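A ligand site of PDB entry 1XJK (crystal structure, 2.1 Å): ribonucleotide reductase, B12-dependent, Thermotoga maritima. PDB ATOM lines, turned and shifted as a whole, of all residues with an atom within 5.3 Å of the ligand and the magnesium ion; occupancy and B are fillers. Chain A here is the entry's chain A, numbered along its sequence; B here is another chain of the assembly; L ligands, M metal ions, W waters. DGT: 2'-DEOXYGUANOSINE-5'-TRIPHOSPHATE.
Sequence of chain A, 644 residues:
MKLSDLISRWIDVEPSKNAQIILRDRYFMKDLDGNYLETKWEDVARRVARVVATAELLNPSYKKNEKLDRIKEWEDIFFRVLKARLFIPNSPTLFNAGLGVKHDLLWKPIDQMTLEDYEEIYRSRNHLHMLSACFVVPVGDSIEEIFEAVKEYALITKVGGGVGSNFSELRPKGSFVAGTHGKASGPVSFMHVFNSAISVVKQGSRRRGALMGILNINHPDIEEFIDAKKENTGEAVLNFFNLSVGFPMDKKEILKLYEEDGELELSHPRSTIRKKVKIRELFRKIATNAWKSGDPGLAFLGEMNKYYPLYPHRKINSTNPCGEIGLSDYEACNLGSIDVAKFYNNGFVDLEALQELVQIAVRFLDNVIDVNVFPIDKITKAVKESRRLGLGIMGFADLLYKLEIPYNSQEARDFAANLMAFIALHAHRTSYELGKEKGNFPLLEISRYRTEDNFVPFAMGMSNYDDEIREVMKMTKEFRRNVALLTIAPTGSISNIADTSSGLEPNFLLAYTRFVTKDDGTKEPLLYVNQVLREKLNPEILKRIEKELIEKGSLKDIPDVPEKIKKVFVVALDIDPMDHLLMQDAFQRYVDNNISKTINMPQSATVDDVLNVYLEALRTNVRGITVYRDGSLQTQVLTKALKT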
ATOM      1  N   ASP A 141      -9.612  -9.148  -3.324  1.00  0.00           N
ATOM      2  CA  ASP A 141      -9.665  -9.380  -4.783  1.00  0.00           C
ATOM      3  C   ASP A 141      -9.246  -8.179  -5.611  1.00  0.00           C
ATOM      4  O   ASP A 141     -10.001  -7.725  -6.475  1.00  0.00           O
ATOM      5  CB  ASP A 141     -11.092  -9.759  -5.183  1.00  0.00           C
ATOM      6  CG  ASP A 141     -11.144 -10.374  -6.548  1.00  0.00           C
ATOM      7  OD1 ASP A 141     -10.112 -10.888  -6.980  1.00  0.00           O
ATOM      8  OD2 ASP A 141     -12.201 -10.294  -7.200  1.00  0.00           O
ATOM      9  N   SER A 142      -8.042  -7.672  -5.381  1.00  0.00           N
ATOM     10  CA  SER A 142      -7.471  -6.595  -6.171  1.00  0.00           C
ATOM     11  C   SER A 142      -5.963  -6.600  -6.135  1.00  0.00           C
ATOM     12  O   SER A 142      -5.362  -7.113  -5.219  1.00  0.00           O
ATOM     13  CB  SER A 142      -8.022  -5.228  -5.719  1.00  0.00           C
ATOM     14  OG  SER A 142      -7.308  -4.791  -4.594  1.00  0.00           O
ATOM     15  N   ILE A 143      -5.342  -5.958  -7.127  1.00  0.00           N
ATOM     16  CA  ILE A 143      -3.890  -5.970  -7.245  1.00  0.00           C
ATOM     17  C   ILE A 143      -3.219  -5.310  -6.059  1.00  0.00           C
ATOM     18  O   ILE A 143      -2.201  -5.776  -5.575  1.00  0.00           O
ATOM     19  CB  ILE A 143      -3.382  -5.286  -8.578  1.00  0.00           C
ATOM     20  CG1 ILE A 143      -3.736  -6.167  -9.751  1.00  0.00           C
ATOM     21  CG2 ILE A 143      -1.844  -5.073  -8.513  1.00  0.00           C
ATOM     22  CD1 ILE A 143      -3.068  -7.515  -9.657  1.00  0.00           C
ATOM     23  N   GLU A 144      -3.752  -4.180  -5.662  1.00  0.00           N
ATOM     24  CA  GLU A 144      -3.287  -3.446  -4.499  1.00  0.00           C
ATOM     25  C   GLU A 144      -3.393  -4.196  -3.154  1.00  0.00           C
ATOM     26  O   GLU A 144      -2.484  -4.153  -2.294  1.00  0.00           O
ATOM     27  CB  GLU A 144      -4.040  -2.120  -4.474  1.00  0.00           C
ATOM     28  CG  GLU A 144      -4.459  -1.610  -3.111  1.00  0.00           C
ATOM     29  CD  GLU A 144      -3.529  -0.576  -2.550  1.00  0.00           C
ATOM     30  OE1 GLU A 144      -3.126   0.335  -3.319  1.00  0.00           O
ATOM     31  OE2 GLU A 144      -3.225  -0.650  -1.330  1.00  0.00           O
ATOM     32  N   ILE A 146      -3.654  -7.602  -2.930  1.00  0.00           N
ATOM     33  CA  ILE A 146      -2.767  -8.746  -3.088  1.00  0.00           C
ATOM     34  C   ILE A 146      -1.366  -8.382  -2.681  1.00  0.00           C
ATOM     35  O   ILE A 146      -0.720  -9.047  -1.863  1.00  0.00           O
ATOM     36  CB  ILE A 146      -2.772  -9.297  -4.568  1.00  0.00           C
ATOM     37  CG1 ILE A 146      -4.021 -10.092  -4.842  1.00  0.00           C
ATOM     38  CG2 ILE A 146      -1.605 -10.274  -4.796  1.00  0.00           C
ATOM     39  CD1 ILE A 146      -4.555  -9.898  -6.216  1.00  0.00           C
ATOM     40  N   LEU A 170      -9.815 -14.067  -4.269  1.00  0.00           N
ATOM     41  CA  LEU A 170      -9.322 -13.801  -5.599  1.00  0.00           C
ATOM     42  C   LEU A 170     -10.154 -14.526  -6.646  1.00  0.00           C
ATOM     43  O   LEU A 170     -10.476 -15.721  -6.489  1.00  0.00           O
ATOM     44  CB  LEU A 170      -7.812 -14.133  -5.736  1.00  0.00           C
ATOM     45  CG  LEU A 170      -6.957 -13.571  -4.568  1.00  0.00           C
ATOM     46  CD1 LEU A 170      -5.513 -13.890  -4.689  1.00  0.00           C
ATOM     47  CD2 LEU A 170      -7.149 -12.034  -4.480  1.00  0.00           C
ATOM     48  N   ARG A 171     -10.518 -13.828  -7.722  1.00  0.00           N
ATOM     49  CA  ARG A 171     -11.431 -14.361  -8.737  1.00  0.00           C
ATOM     50  C   ARG A 171     -10.701 -15.363  -9.605  1.00  0.00           C
ATOM     51  O   ARG A 171      -9.490 -15.212  -9.827  1.00  0.00           O
ATOM     52  CB  ARG A 171     -12.072 -13.195  -9.523  1.00  0.00           C
ATOM     53  CG  ARG A 171     -11.162 -12.449 -10.540  1.00  0.00           C
ATOM     54  CD  ARG A 171     -11.775 -11.128 -11.033  1.00  0.00           C
ATOM     55  NE  ARG A 171     -11.974 -10.108  -9.993  1.00  0.00           N
ATOM     56  CZ  ARG A 171     -12.213  -8.823 -10.249  1.00  0.00           C
ATOM     57  NH1 ARG A 171     -12.283  -8.386 -11.515  1.00  0.00           N
ATOM     58  NH2 ARG A 171     -12.364  -7.946  -9.255  1.00  0.00           N
ATOM     59  N   PHE A 176     -13.088 -11.996 -15.655  1.00  0.00           N
ATOM     60  CA  PHE A 176     -13.206 -10.633 -16.178  1.00  0.00           C
ATOM     61  C   PHE A 176     -12.585  -9.559 -15.278  1.00  0.00           C
ATOM     62  O   PHE A 176     -12.891  -9.469 -14.074  1.00  0.00           O
ATOM     63  CB  PHE A 176     -14.698 -10.332 -16.458  1.00  0.00           C
ATOM     64  CG  PHE A 176     -14.995  -8.899 -16.799  1.00  0.00           C
ATOM     65  CD1 PHE A 176     -14.877  -8.440 -18.109  1.00  0.00           C
ATOM     66  CD2 PHE A 176     -15.417  -8.002 -15.810  1.00  0.00           C
ATOM     67  CE1 PHE A 176     -15.140  -7.103 -18.433  1.00  0.00           C
ATOM     68  CE2 PHE A 176     -15.687  -6.645 -16.104  1.00  0.00           C
ATOM     69  CZ  PHE A 176     -15.547  -6.203 -17.424  1.00  0.00           C
ATOM     70  N   VAL A 177     -11.757  -8.705 -15.881  1.00  0.00           N
ATOM     71  CA  VAL A 177     -11.205  -7.556 -15.126  1.00  0.00           C
ATOM     72  C   VAL A 177     -11.742  -6.256 -15.693  1.00  0.00           C
ATOM     73  O   VAL A 177     -11.573  -5.982 -16.880  1.00  0.00           O
ATOM     74  CB  VAL A 177      -9.631  -7.538 -15.089  1.00  0.00           C
ATOM     75  CG1 VAL A 177      -9.125  -6.350 -14.276  1.00  0.00           C
ATOM     76  CG2 VAL A 177      -9.067  -8.851 -14.541  1.00  0.00           C
ATOM     77  N   ALA A 178     -12.398  -5.463 -14.844  1.00  0.00           N
ATOM     78  CA  ALA A 178     -13.068  -4.247 -15.303  1.00  0.00           C
ATOM     79  C   ALA A 178     -12.145  -3.277 -16.013  1.00  0.00           C
ATOM     80  O   ALA A 178     -11.055  -2.976 -15.525  1.00  0.00           O
ATOM     81  CB  ALA A 178     -13.807  -3.528 -14.170  1.00  0.00           C
ATOM     82  N   LYS A 183      -7.683 -10.534 -18.627  1.00  0.00           N
ATOM     83  CA  LYS A 183      -8.293 -11.462 -17.656  1.00  0.00           C
ATOM     84  C   LYS A 183      -7.494 -11.676 -16.350  1.00  0.00           C
ATOM     85  O   LYS A 183      -6.281 -11.508 -16.318  1.00  0.00           O
ATOM     86  CB  LYS A 183      -8.657 -12.781 -18.344  1.00  0.00           C
ATOM     87  CG  LYS A 183      -9.687 -12.631 -19.491  1.00  0.00           C
ATOM     88  CD  LYS A 183      -9.856 -13.957 -20.256  1.00  0.00           C
ATOM     89  CE  LYS A 183      -9.978 -13.737 -21.770  1.00  0.00           C
ATOM     90  NZ  LYS A 183      -8.651 -13.452 -22.410  1.00  0.00           N
ATOM     91  N   ALA A 184      -8.198 -11.980 -15.261  1.00  0.00           N
ATOM     92  CA  ALA A 184      -7.561 -12.234 -13.967  1.00  0.00           C
ATOM     93  C   ALA A 184      -6.761 -13.514 -14.046  1.00  0.00           C
ATOM     94  O   ALA A 184      -7.144 -14.465 -14.748  1.00  0.00           O
ATOM     95  CB  ALA A 184      -8.559 -12.307 -12.889  1.00  0.00           C
ATOM     96  N   SER A 185      -5.610 -13.539 -13.367  1.00  0.00           N
ATOM     97  CA  SER A 185      -4.758 -14.722 -13.439  1.00  0.00           C
ATOM     98  C   SER A 185      -5.136 -15.818 -12.406  1.00  0.00           C
ATOM     99  O   SER A 185      -4.792 -16.967 -12.595  1.00  0.00           O
ATOM    100  CB  SER A 185      -3.267 -14.331 -13.382  1.00  0.00           C
ATOM    101  OG  SER A 185      -2.964 -13.703 -12.158  1.00  0.00           O
ATOM    102  N   SER A 189      -1.884 -18.317  -9.158  1.00  0.00           N
ATOM    103  CA  SER A 189      -0.847 -17.483  -9.757  1.00  0.00           C
ATOM    104  C   SER A 189      -0.201 -16.538  -8.766  1.00  0.00           C
ATOM    105  O   SER A 189       0.990 -16.411  -8.714  1.00  0.00           O
ATOM    106  CB  SER A 189      -1.349 -16.705 -10.992  1.00  0.00           C
ATOM    107  OG  SER A 189      -2.231 -15.671 -10.637  1.00  0.00           O
ATOM    108  N   PHE A 190      -0.997 -15.871  -7.959  1.00  0.00           N
ATOM    109  CA  PHE A 190      -0.438 -14.900  -6.979  1.00  0.00           C
ATOM    110  C   PHE A 190       0.201 -15.595  -5.804  1.00  0.00           C
ATOM    111  O   PHE A 190       1.053 -15.009  -5.128  1.00  0.00           O
ATOM    112  CB  PHE A 190      -1.498 -13.943  -6.508  1.00  0.00           C
ATOM    113  CG  PHE A 190      -2.044 -13.102  -7.615  1.00  0.00           C
ATOM    114  CD1 PHE A 190      -1.282 -12.075  -8.141  1.00  0.00           C
ATOM    115  CD2 PHE A 190      -3.261 -13.405  -8.201  1.00  0.00           C
ATOM    116  CE1 PHE A 190      -1.722 -11.325  -9.189  1.00  0.00           C
ATOM    117  CE2 PHE A 190      -3.749 -12.643  -9.228  1.00  0.00           C
ATOM    118  CZ  PHE A 190      -2.977 -11.618  -9.751  1.00  0.00           C
ATOM    119  N   HIS B 127      -9.110   5.966 -13.106  1.00  0.00           N
ATOM    120  CA  HIS B 127      -7.822   5.586 -12.534  1.00  0.00           C
ATOM    121  C   HIS B 127      -6.925   4.807 -13.527  1.00  0.00           C
ATOM    122  O   HIS B 127      -5.728   4.587 -13.316  1.00  0.00           O
ATOM    123  CB  HIS B 127      -8.118   4.735 -11.264  1.00  0.00           C
ATOM    124  CG  HIS B 127      -8.869   3.468 -11.567  1.00  0.00           C
ATOM    125  ND1 HIS B 127      -8.287   2.213 -11.464  1.00  0.00           N
ATOM    126  CD2 HIS B 127     -10.117   3.261 -12.052  1.00  0.00           C
ATOM    127  CE1 HIS B 127      -9.157   1.295 -11.842  1.00  0.00           C
ATOM    128  NE2 HIS B 127     -10.281   1.904 -12.209  1.00  0.00           N
ATOM    129  N   LEU B 128      -7.500   4.391 -14.646  1.00  0.00           N
ATOM    130  CA  LEU B 128      -6.727   3.671 -15.626  1.00  0.00           C
ATOM    131  C   LEU B 128      -6.240   4.651 -16.715  1.00  0.00           C
ATOM    132  O   LEU B 128      -5.523   4.259 -17.649  1.00  0.00           O
ATOM    133  CB  LEU B 128      -7.593   2.577 -16.246  1.00  0.00           C
ATOM    134  CG  LEU B 128      -8.111   1.417 -15.392  1.00  0.00           C
ATOM    135  CD1 LEU B 128      -8.286   0.288 -16.373  1.00  0.00           C
ATOM    136  CD2 LEU B 128      -7.112   0.996 -14.229  1.00  0.00           C
ATOM    137  N   LYS B 158       0.415  -2.751 -14.060  1.00  0.00           N
ATOM    138  CA  LYS B 158      -1.023  -2.950 -14.324  1.00  0.00           C
ATOM    139  C   LYS B 158      -1.583  -1.942 -15.290  1.00  0.00           C
ATOM    140  O   LYS B 158      -2.235  -2.317 -16.258  1.00  0.00           O
ATOM    141  CB  LYS B 158      -1.857  -2.929 -13.033  1.00  0.00           C
ATOM    142  CG  LYS B 158      -3.271  -3.469 -13.221  1.00  0.00           C
ATOM    143  CD  LYS B 158      -4.184  -3.059 -12.041  1.00  0.00           C
ATOM    144  CE  LYS B 158      -5.668  -3.302 -12.379  1.00  0.00           C
ATOM    145  NZ  LYS B 158      -6.550  -2.234 -11.786  1.00  0.00           N
ATOM    146  N   VAL B 200       3.780 -12.395 -12.939  1.00  0.00           N
ATOM    147  CA  VAL B 200       2.379 -12.754 -12.677  1.00  0.00           C
ATOM    148  C   VAL B 200       1.447 -11.659 -13.167  1.00  0.00           C
ATOM    149  O   VAL B 200       0.461 -11.946 -13.829  1.00  0.00           O
ATOM    150  CB  VAL B 200       2.058 -13.100 -11.162  1.00  0.00           C
ATOM    151  CG1 VAL B 200       0.558 -13.097 -10.903  1.00  0.00           C
ATOM    152  CG2 VAL B 200       2.607 -14.431 -10.769  1.00  0.00           C
ATOM    153  N   VAL B 201       1.738 -10.416 -12.800  1.00  0.00           N
ATOM    154  CA  VAL B 201       0.939  -9.308 -13.266  1.00  0.00           C
ATOM    155  C   VAL B 201       0.849  -9.287 -14.800  1.00  0.00           C
ATOM    156  O   VAL B 201      -0.234  -9.080 -15.322  1.00  0.00           O
ATOM    157  CB  VAL B 201       1.411  -7.961 -12.733  1.00  0.00           C
ATOM    158  CG1 VAL B 201       0.588  -6.870 -13.357  1.00  0.00           C
ATOM    159  CG2 VAL B 201       1.279  -7.923 -11.214  1.00  0.00           C
ATOM    160  N   LYS B 202       1.942  -9.548 -15.501  1.00  0.00           N
ATOM    161  CA  LYS B 202       1.933  -9.615 -16.961  1.00  0.00           C
ATOM    162  C   LYS B 202       1.502 -10.942 -17.609  1.00  0.00           C
ATOM    163  O   LYS B 202       1.600 -11.087 -18.817  1.00  0.00           O
ATOM    164  CB  LYS B 202       3.271  -9.121 -17.549  1.00  0.00           C
ATOM    165  CG  LYS B 202       3.426  -7.613 -17.337  1.00  0.00           C
ATOM    166  CD  LYS B 202       4.116  -6.921 -18.512  1.00  0.00           C
ATOM    167  CE  LYS B 202       3.421  -5.571 -18.780  1.00  0.00           C
ATOM    168  NZ  LYS B 202       4.339  -4.466 -19.232  1.00  0.00           N
ATOM    169  N   GLN B 203       1.017 -11.900 -16.836  1.00  0.00           N
ATOM    170  CA  GLN B 203       0.315 -13.057 -17.432  1.00  0.00           C
ATOM    171  C   GLN B 203      -1.224 -12.898 -17.375  1.00  0.00           C
ATOM    172  O   GLN B 203      -1.758 -11.781 -17.486  1.00  0.00           O
ATOM    173  CB  GLN B 203       0.733 -14.361 -16.763  1.00  0.00           C
ATOM    174  CG  GLN B 203       0.359 -14.434 -15.297  1.00  0.00           C
ATOM    175  CD  GLN B 203      -0.001 -15.835 -14.852  1.00  0.00           C
ATOM    176  OE1 GLN B 203      -1.079 -16.352 -15.177  1.00  0.00           O
ATOM    177  NE2 GLN B 203       0.889 -16.464 -14.084  1.00  0.00           N
HETATM  178  PG  DGT L   1     -12.247  -4.746 -11.290  1.00  0.00           P
HETATM  179  O1G DGT L   1     -12.823  -5.625 -12.305  1.00  0.00           O
HETATM  180  O2G DGT L   1     -11.721  -5.361 -10.030  1.00  0.00           O
HETATM  181  O3G DGT L   1     -13.181  -3.473 -10.812  1.00  0.00           O
HETATM  182  O3B DGT L   1     -10.985  -4.206 -12.108  1.00  0.00           O
HETATM  183  PB  DGT L   1      -9.737  -3.507 -11.329  1.00  0.00           P
HETATM  184  O1B DGT L   1      -9.020  -2.689 -12.343  1.00  0.00           O
HETATM  185  O2B DGT L   1     -10.267  -2.857 -10.086  1.00  0.00           O
HETATM  186  O3A DGT L   1      -8.725  -4.728 -10.971  1.00  0.00           O
HETATM  187  PA  DGT L   1      -8.191  -5.164  -9.473  1.00  0.00           P
HETATM  188  O1A DGT L   1      -9.224  -4.965  -8.437  1.00  0.00           O
HETATM  189  O2A DGT L   1      -6.851  -4.599  -9.245  1.00  0.00           O
HETATM  190  O5' DGT L   1      -8.069  -6.766  -9.758  1.00  0.00           O
HETATM  191  C5' DGT L   1      -9.103  -7.647  -9.566  1.00  0.00           C
HETATM  192  C4' DGT L   1      -8.627  -9.138  -9.624  1.00  0.00           C
HETATM  193  O4' DGT L   1      -8.117  -9.240 -10.964  1.00  0.00           O
HETATM  194  C3' DGT L   1      -7.508  -9.624  -8.654  1.00  0.00           C
HETATM  195  O3' DGT L   1      -7.602 -11.066  -8.449  1.00  0.00           O
HETATM  196  C2' DGT L   1      -6.336  -9.315  -9.520  1.00  0.00           C
HETATM  197  C1' DGT L   1      -6.826  -9.680 -10.967  1.00  0.00           C
HETATM  198  N9  DGT L   1      -6.064  -8.799 -11.900  1.00  0.00           N
HETATM  199  C8  DGT L   1      -6.354  -7.511 -12.163  1.00  0.00           C
HETATM  200  N7  DGT L   1      -5.465  -6.968 -12.977  1.00  0.00           N
HETATM  201  C5  DGT L   1      -4.610  -7.955 -13.263  1.00  0.00           C
HETATM  202  C6  DGT L   1      -3.474  -7.947 -14.047  1.00  0.00           C
HETATM  203  O6  DGT L   1      -3.202  -6.897 -14.593  1.00  0.00           O
HETATM  204  N1  DGT L   1      -2.680  -9.101 -14.188  1.00  0.00           N
HETATM  205  C2  DGT L   1      -3.087 -10.233 -13.463  1.00  0.00           C
HETATM  206  N2  DGT L   1      -2.401 -11.335 -13.577  1.00  0.00           N
HETATM  207  N3  DGT L   1      -4.194 -10.232 -12.699  1.00  0.00           N
HETATM  208  C4  DGT L   1      -4.975  -9.113 -12.580  1.00  0.00           C
HETATM  209 MG    MG M   1     -10.943  -4.081  -8.436  1.00  0.00          MG
HETATM  210  O   HOH W   1     -12.779  -0.602 -11.037  1.00  0.00           O
HETATM  211  O   HOH W   2      -5.832  -2.367  -7.542  1.00  0.00           O
HETATM  212  O   HOH W   3      -7.251 -13.399  -9.712  1.00  0.00           O
HETATM  213  O   HOH W   4     -10.633   0.164  -9.135  1.00  0.00           O
HETATM  214  O   HOH W   5      -0.983  -6.582 -16.900  1.00  0.00           O
HETATM  215  O   HOH W   6     -11.568  -5.419  -6.606  1.00  0.00           O
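The side-chain amino group (NZ) of Lys 158 of chain B lies within salt-bridge range of an oxygen (O1B) of the ligand, 2.6 Å away.
An oxygen (O1G) of the ligand is in hydrogen-bond range of the backbone NH (N) of Ala 178, 2.6 Å away.
O of Val 201 of chain B is in hydrogen-bond range of N1 of the ligand (2.7 Å).
An oxygen (O1G) of the ligand lies within salt-bridge range of the guanidinium group (NH1) of Arg 171.
The side-chain hydroxyl (OG) of Ser 185 is in hydrogen-bond range of a nitrogen (N2) of the ligand.
O3' of the ligand is in hydrogen-bond range of OD1 of Asp 141, 2.9 Å away.
N of Ile 143 is in hydrogen-bond range of O2A of the ligand, at 2.9 Å.
The backbone carbonyl oxygen (O) of Val 200 of chain B lies within hydrogen-bond range of a nitrogen (N2) of the ligand, 2.9 Å away.
The side-chain carboxylate (OD2) of Asp 141 lies within salt-bridge range of the guanidinium group (NE) of Arg 171, at 2.8 Å.
The guanidinium group (NH1) of Arg 171 is in hydrogen-bond range of the backbone carbonyl oxygen (O) of Phe 176.
The side-chain hydroxyl (OG) of Ser 185 is in hydrogen-bond range of the side-chain hydroxyl (OG) of Ser 189, 2.6 Å away.
Merely in contact with the ligand: Ser 142 (3.0 Å), Ile 146 (3.8 Å), Val 177 (3.6 Å), Ala 184 (3.6 Å), Phe 190 (3.5 Å) and Gln 203 of chain B (3.99 Å).
No residue comes within 4 Å of the magnesium ion.
The nearest printed residue that does not touch the magnesium ion is Ser 142 (4.2 Å).
The magnesium ion is bound by O1A of the ligand (1.9 Å).
The magnesium ion is bound by O2B of the ligand (2.2 Å).
The magnesium ion is bound by O2G of the ligand (2.2 Å).
Water W6 is bound to the magnesium ion (2.4 Å).
The magnesium ion has four donor atoms within binding distance.
Water W3 lies within hydrogen-bond range of an oxygen (O3') of the ligand (2.7 Å) and the backbone carbonyl oxygen of Arg 171 (2.9 Å).
Water W2 bridges an oxygen (O2A) of the ligand and the backbone NH (N) of Glu 144.
Water W5 bridges O of Val 201 of chain B and O6 of the ligand.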
